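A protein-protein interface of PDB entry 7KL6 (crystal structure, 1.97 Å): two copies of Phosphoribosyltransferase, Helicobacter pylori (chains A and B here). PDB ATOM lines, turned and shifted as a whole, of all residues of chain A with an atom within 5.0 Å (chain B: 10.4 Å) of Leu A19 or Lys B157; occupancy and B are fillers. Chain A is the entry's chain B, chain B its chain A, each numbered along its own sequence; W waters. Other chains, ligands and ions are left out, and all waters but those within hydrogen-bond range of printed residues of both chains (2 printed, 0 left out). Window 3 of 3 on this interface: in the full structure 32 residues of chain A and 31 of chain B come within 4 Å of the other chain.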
ATOM      1  N   LEU A  15      27.957  25.720 -22.118  1.00  0.00           N
ATOM      2  CA  LEU A  15      28.135  24.521 -22.947  1.00  0.00           C
ATOM      3  C   LEU A  15      26.835  24.132 -23.649  1.00  0.00           C
ATOM      4  O   LEU A  15      26.822  23.832 -24.850  1.00  0.00           O
ATOM      5  CB  LEU A  15      28.603  23.339 -22.087  1.00  0.00           C
ATOM      6  CG  LEU A  15      30.070  23.117 -21.727  1.00  0.00           C
ATOM      7  CD1 LEU A  15      30.221  21.795 -20.938  1.00  0.00           C
ATOM      8  CD2 LEU A  15      30.977  23.128 -22.966  1.00  0.00           C
ATOM      9  N   LYS A  16      25.743  24.068 -22.884  1.00  0.00           N
ATOM     10  CA  LYS A  16      24.424  23.769 -23.437  1.00  0.00           C
ATOM     11  C   LYS A  16      24.044  24.754 -24.533  1.00  0.00           C
ATOM     12  O   LYS A  16      23.602  24.356 -25.620  1.00  0.00           O
ATOM     13  CB  LYS A  16      23.388  23.794 -22.308  1.00  0.00           C
ATOM     14  CG  LYS A  16      21.938  23.495 -22.722  1.00  0.00           C
ATOM     15  CD  LYS A  16      21.083  23.231 -21.482  1.00  0.00           C
ATOM     16  CE  LYS A  16      19.595  23.230 -21.805  1.00  0.00           C
ATOM     17  NZ  LYS A  16      18.796  22.616 -20.699  1.00  0.00           N
ATOM     18  N   ASP A  17      24.199  26.053 -24.266  1.00  0.00           N
ATOM     19  CA  ASP A  17      23.827  27.048 -25.262  1.00  0.00           C
ATOM     20  C   ASP A  17      24.738  26.996 -26.479  1.00  0.00           C
ATOM     21  O   ASP A  17      24.300  27.315 -27.587  1.00  0.00           O
ATOM     22  CB  ASP A  17      23.895  28.462 -24.686  1.00  0.00           C
ATOM     23  CG  ASP A  17      22.754  28.774 -23.750  1.00  0.00           C
ATOM     24  OD1 ASP A  17      21.703  28.107 -23.843  1.00  0.00           O
ATOM     25  OD2 ASP A  17      22.914  29.711 -22.934  1.00  0.00           O
ATOM     26  N   SER A  18      26.015  26.667 -26.287  1.00  0.00           N
ATOM     27  CA  SER A  18      26.931  26.656 -27.427  1.00  0.00           C
ATOM     28  C   SER A  18      26.508  25.606 -28.447  1.00  0.00           C
ATOM     29  O   SER A  18      26.638  25.810 -29.663  1.00  0.00           O
ATOM     30  CB  SER A  18      28.354  26.387 -26.943  1.00  0.00           C
ATOM     31  OG  SER A  18      28.902  27.564 -26.375  1.00  0.00           O
ATOM     32  N   LEU A  19      25.996  24.469 -27.968  1.00  0.00           N
ATOM     33  CA  LEU A  19      25.484  23.450 -28.879  1.00  0.00           C
ATOM     34  C   LEU A  19      24.299  23.979 -29.670  1.00  0.00           C
ATOM     35  O   LEU A  19      24.148  23.681 -30.862  1.00  0.00           O
ATOM     36  CB  LEU A  19      25.070  22.206 -28.101  1.00  0.00           C
ATOM     37  CG  LEU A  19      26.146  21.224 -27.680  1.00  0.00           C
ATOM     38  CD1 LEU A  19      25.468  20.031 -27.006  1.00  0.00           C
ATOM     39  CD2 LEU A  19      26.957  20.759 -28.914  1.00  0.00           C
ATOM     40  N   GLU A  20      23.434  24.743 -29.016  1.00  0.00           N
ATOM     41  CA  GLU A  20      22.290  25.302 -29.722  1.00  0.00           C
ATOM     42  C   GLU A  20      22.752  26.358 -30.710  1.00  0.00           C
ATOM     43  O   GLU A  20      22.245  26.433 -31.832  1.00  0.00           O
ATOM     44  CB  GLU A  20      21.286  25.873 -28.715  1.00  0.00           C
ATOM     45  CG  GLU A  20      20.038  26.449 -29.343  1.00  0.00           C
ATOM     46  CD  GLU A  20      19.237  25.392 -30.107  1.00  0.00           C
ATOM     47  OE1 GLU A  20      19.311  24.198 -29.744  1.00  0.00           O
ATOM     48  OE2 GLU A  20      18.548  25.760 -31.083  1.00  0.00           O
ATOM     49  N   LEU A  21      23.750  27.153 -30.321  1.00  0.00           N
ATOM     50  CA  LEU A  21      24.311  28.145 -31.231  1.00  0.00           C
ATOM     51  C   LEU A  21      24.874  27.485 -32.476  1.00  0.00           C
ATOM     52  O   LEU A  21      24.656  27.965 -33.593  1.00  0.00           O
ATOM     53  CB  LEU A  21      25.400  28.953 -30.526  1.00  0.00           C
ATOM     54  CG  LEU A  21      25.814  30.194 -31.319  1.00  0.00           C
ATOM     55  CD1 LEU A  21      24.559  31.014 -31.548  1.00  0.00           C
ATOM     56  CD2 LEU A  21      26.836  31.020 -30.558  1.00  0.00           C
ATOM     57  N   VAL A  22      25.618  26.388 -32.295  1.00  0.00           N
ATOM     58  CA  VAL A  22      26.144  25.624 -33.428  1.00  0.00           C
ATOM     59  C   VAL A  22      25.007  25.222 -34.360  1.00  0.00           C
ATOM     60  O   VAL A  22      25.090  25.354 -35.592  1.00  0.00           O
ATOM     61  CB  VAL A  22      26.900  24.384 -32.914  1.00  0.00           C
ATOM     62  CG1 VAL A  22      27.093  23.355 -34.045  1.00  0.00           C
ATOM     63  CG2 VAL A  22      28.269  24.795 -32.315  1.00  0.00           C
ATOM     64  N   LYS A  23      23.937  24.695 -33.780  1.00  0.00           N
ATOM     65  CA  LYS A  23      22.814  24.232 -34.582  1.00  0.00           C
ATOM     66  C   LYS A  23      22.198  25.376 -35.372  1.00  0.00           C
ATOM     67  O   LYS A  23      21.915  25.241 -36.569  1.00  0.00           O
ATOM     68  CB  LYS A  23      21.780  23.569 -33.678  1.00  0.00           C
ATOM     69  CG  LYS A  23      20.804  22.708 -34.439  1.00  0.00           C
ATOM     70  CD  LYS A  23      20.298  21.548 -33.584  1.00  0.00           C
ATOM     71  CE  LYS A  23      19.501  22.015 -32.383  1.00  0.00           C
ATOM     72  NZ  LYS A  23      18.689  20.891 -31.815  1.00  0.00           N
ATOM     73  N   HIS A  52      35.203  22.844 -32.101  1.00  0.00           N
ATOM     74  CA  HIS A  52      34.073  21.979 -32.446  1.00  0.00           C
ATOM     75  C   HIS A  52      33.964  21.764 -33.953  1.00  0.00           C
ATOM     76  O   HIS A  52      33.662  20.653 -34.410  1.00  0.00           O
ATOM     77  CB  HIS A  52      32.771  22.571 -31.912  1.00  0.00           C
ATOM     78  CG  HIS A  52      31.626  21.612 -31.958  1.00  0.00           C
ATOM     79  ND1 HIS A  52      31.506  20.568 -31.064  1.00  0.00           N
ATOM     80  CD2 HIS A  52      30.547  21.542 -32.773  1.00  0.00           C
ATOM     81  CE1 HIS A  52      30.406  19.886 -31.340  1.00  0.00           C
ATOM     82  NE2 HIS A  52      29.806  20.457 -32.371  1.00  0.00           N
ATOM     83  N   GLU B 150      38.376  21.385 -25.826  1.00  0.00           N
ATOM     84  CA  GLU B 150      38.424  20.453 -26.954  1.00  0.00           C
ATOM     85  C   GLU B 150      37.267  19.444 -26.920  1.00  0.00           C
ATOM     86  O   GLU B 150      36.701  19.103 -27.973  1.00  0.00           O
ATOM     87  CB  GLU B 150      39.745  19.683 -26.912  1.00  0.00           C
ATOM     88  CG  GLU B 150      40.978  20.465 -27.310  1.00  0.00           C
ATOM     89  CD  GLU B 150      42.294  19.699 -27.066  1.00  0.00           C
ATOM     90  OE1 GLU B 150      42.310  18.675 -26.312  1.00  0.00           O
ATOM     91  OE2 GLU B 150      43.329  20.174 -27.594  1.00  0.00           O
ATOM     92  N   VAL B 151      36.924  18.922 -25.733  1.00  0.00           N
ATOM     93  CA  VAL B 151      36.111  17.705 -25.650  1.00  0.00           C
ATOM     94  C   VAL B 151      34.754  17.891 -24.976  1.00  0.00           C
ATOM     95  O   VAL B 151      33.824  17.115 -25.239  1.00  0.00           O
ATOM     96  CB  VAL B 151      36.872  16.564 -24.935  1.00  0.00           C
ATOM     97  CG1 VAL B 151      38.164  16.176 -25.700  1.00  0.00           C
ATOM     98  CG2 VAL B 151      37.150  16.894 -23.447  1.00  0.00           C
ATOM     99  N   ASP B 152      34.618  18.878 -24.084  1.00  0.00           N
ATOM    100  CA  ASP B 152      33.398  18.937 -23.273  1.00  0.00           C
ATOM    101  C   ASP B 152      32.156  19.087 -24.137  1.00  0.00           C
ATOM    102  O   ASP B 152      31.090  18.558 -23.811  1.00  0.00           O
ATOM    103  CB  ASP B 152      33.461  20.093 -22.281  1.00  0.00           C
ATOM    104  CG  ASP B 152      34.233  19.745 -21.022  1.00  0.00           C
ATOM    105  OD1 ASP B 152      34.956  18.723 -21.020  1.00  0.00           O
ATOM    106  OD2 ASP B 152      34.123  20.518 -20.041  1.00  0.00           O
ATOM    107  N   LEU B 153      32.271  19.818 -25.236  1.00  0.00           N
ATOM    108  CA  LEU B 153      31.090  20.152 -26.008  1.00  0.00           C
ATOM    109  C   LEU B 153      30.650  18.967 -26.859  1.00  0.00           C
ATOM    110  O   LEU B 153      29.456  18.627 -26.895  1.00  0.00           O
ATOM    111  CB  LEU B 153      31.405  21.400 -26.825  1.00  0.00           C
ATOM    112  CG  LEU B 153      30.385  22.173 -27.611  1.00  0.00           C
ATOM    113  CD1 LEU B 153      29.380  22.700 -26.582  1.00  0.00           C
ATOM    114  CD2 LEU B 153      31.095  23.358 -28.230  1.00  0.00           C
ATOM    115  N   LYS B 154      31.603  18.263 -27.480  1.00  0.00           N
ATOM    116  CA  LYS B 154      31.219  17.040 -28.182  1.00  0.00           C
ATOM    117  C   LYS B 154      30.780  15.949 -27.213  1.00  0.00           C
ATOM    118  O   LYS B 154      29.941  15.116 -27.568  1.00  0.00           O
ATOM    119  CB  LYS B 154      32.359  16.540 -29.077  1.00  0.00           C
ATOM    120  CG  LYS B 154      33.698  16.355 -28.389  1.00  0.00           C
ATOM    121  CD  LYS B 154      34.742  15.778 -29.361  1.00  0.00           C
ATOM    122  CE  LYS B 154      34.972  16.692 -30.563  1.00  0.00           C
ATOM    123  NZ  LYS B 154      35.583  18.032 -30.220  1.00  0.00           N
ATOM    124  N   ASN B 155      31.330  15.925 -25.993  1.00  0.00           N
ATOM    125  CA  ASN B 155      30.881  14.927 -25.022  1.00  0.00           C
ATOM    126  C   ASN B 155      29.452  15.197 -24.578  1.00  0.00           C
ATOM    127  O   ASN B 155      28.655  14.263 -24.446  1.00  0.00           O
ATOM    128  CB  ASN B 155      31.811  14.888 -23.806  1.00  0.00           C
ATOM    129  CG  ASN B 155      33.144  14.211 -24.097  1.00  0.00           C
ATOM    130  OD1 ASN B 155      33.307  13.512 -25.103  1.00  0.00           O
ATOM    131  ND2 ASN B 155      34.102  14.409 -23.203  1.00  0.00           N
ATOM    132  N   LEU B 156      29.116  16.466 -24.322  1.00  0.00           N
ATOM    133  CA  LEU B 156      27.740  16.806 -23.962  1.00  0.00           C
ATOM    134  C   LEU B 156      26.779  16.448 -25.092  1.00  0.00           C
ATOM    135  O   LEU B 156      25.685  15.937 -24.848  1.00  0.00           O
ATOM    136  CB  LEU B 156      27.635  18.297 -23.631  1.00  0.00           C
ATOM    137  CG  LEU B 156      26.201  18.807 -23.378  1.00  0.00           C
ATOM    138  CD1 LEU B 156      25.636  18.173 -22.126  1.00  0.00           C
ATOM    139  CD2 LEU B 156      26.125  20.342 -23.284  1.00  0.00           C
ATOM    140  N   LYS B 157      27.180  16.700 -26.339  1.00  0.00           N
ATOM    141  CA  LYS B 157      26.295  16.427 -27.464  1.00  0.00           C
ATOM    142  C   LYS B 157      26.010  14.937 -27.592  1.00  0.00           C
ATOM    143  O   LYS B 157      24.883  14.536 -27.901  1.00  0.00           O
ATOM    144  CB  LYS B 157      26.922  16.962 -28.758  1.00  0.00           C
ATOM    145  CG  LYS B 157      26.078  16.707 -30.022  1.00  0.00           C
ATOM    146  CD  LYS B 157      26.900  16.979 -31.275  1.00  0.00           C
ATOM    147  CE  LYS B 157      26.189  16.519 -32.552  1.00  0.00           C
ATOM    148  NZ  LYS B 157      27.103  16.600 -33.738  1.00  0.00           N
ATOM    149  N   SER B 158      27.013  14.106 -27.325  1.00  0.00           N
ATOM    150  CA  SER B 158      26.986  12.680 -27.620  1.00  0.00           C
ATOM    151  C   SER B 158      26.543  11.821 -26.442  1.00  0.00           C
ATOM    152  O   SER B 158      26.686  10.592 -26.501  1.00  0.00           O
ATOM    153  CB  SER B 158      28.373  12.227 -28.069  1.00  0.00           C
ATOM    154  OG  SER B 158      29.308  12.438 -27.027  1.00  0.00           O
ATOM    155  N   HIS B 159      26.030  12.432 -25.378  1.00  0.00           N
ATOM    156  CA  HIS B 159      25.594  11.690 -24.199  1.00  0.00           C
ATOM    157  C   HIS B 159      24.276  12.263 -23.700  1.00  0.00           C
ATOM    158  O   HIS B 159      23.632  13.037 -24.407  1.00  0.00           O
ATOM    159  CB  HIS B 159      26.654  11.727 -23.091  1.00  0.00           C
ATOM    160  CG  HIS B 159      27.941  11.054 -23.456  1.00  0.00           C
ATOM    161  ND1 HIS B 159      29.112  11.748 -23.681  1.00  0.00           N
ATOM    162  CD2 HIS B 159      28.244   9.744 -23.625  1.00  0.00           C
ATOM    163  CE1 HIS B 159      30.078  10.896 -23.976  1.00  0.00           C
ATOM    164  NE2 HIS B 159      29.578   9.674 -23.951  1.00  0.00           N
HETATM  165  O   HOH W   1      27.222  19.835 -33.269  1.00  0.00           O
HETATM  166  O   HOH W   2      33.834  19.790 -29.135  1.00  0.00           O
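CD1 of Leu A15 touches CB of Asp B152, 3.9 Å away. CD1 of Leu B153 touches O of Leu A15 (3.3 Å). Leu A15 touches Leu B156. Lys A16 touches Leu B156. Ser A18 touches Leu B153. CD1 of Leu B153 touches CG of Leu A19, 3.7 Å away. CD2 of Leu B156 touches CD1 of Leu A19 (3.8 Å). Leu A19 touches Lys B157. Leu B153 touches His A52 (CG to ND1, 3.97 Å).
Of the 10 printed residues of chain B, 4 touch a printed residue of chain A. Hydrophobic or aromatic side chains of chain B that line the printed part of chain A: Leu B153 and Leu B156. Along chain B the printed residues that touch a printed residue of chain A span positions 152 to 157. Of the 10 printed residues of chain A, 5 touch a printed residue of chain B. Hydrophobic or aromatic side chains of chain A that line the printed part of chain B: Leu A15, Leu A19 and His A52. Among the printed residues, no Asp or Glu carboxylate lies within 4 Å of a Lys or Arg side-chain nitrogen of the other chain.
No position is printed for both chains. Of the 9 pairs that touch across the chains among the printed residues, none has its exchanged pair printed and touching as well.
Of the printed residues of chain B, Leu A15 touches Asp B152, Leu B153 and Leu B156. Printed residues of chain B within 4 Å of Lys A16: Leu B156 (3.8 Å). Of chain B, only Leu B153 (3.7 Å), Leu B156 (3.8 Å) and Lys B157 (3.7 Å) come within 4 Å of Leu A19. Val A22 touches none of the printed residues of chain B. No residue of chain B comes within 4 Å of Lys A23. Of the printed residues of chain B, His A52 touches Leu B153 (3.97 Å). Glu B150 touches none of the printed residues of chain A. Printed residues of chain A within 4 Å of Leu B153: Leu A15 (3.3 Å), Ser A18 (3.8 Å), Leu A19 (3.7 Å) and His A52 (3.97 Å). Asn B155 touches none of the printed residues of chain A. Of the printed residues of chain A, Leu B156 touches Leu A15, Lys A16 and Leu A19. Lys B157 touches just one residue of chain A: Leu A19.
Water W2 lies within hydrogen-bond range of the side-chain amino group (NZ) of Lys B154, a ring nitrogen (ND1) of His A52 and the backbone carbonyl oxygen (O) of Glu B150. Water W1 bridges NE2 of His A52 (2.8 Å) and NZ of Lys B157 (3.3 Å).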
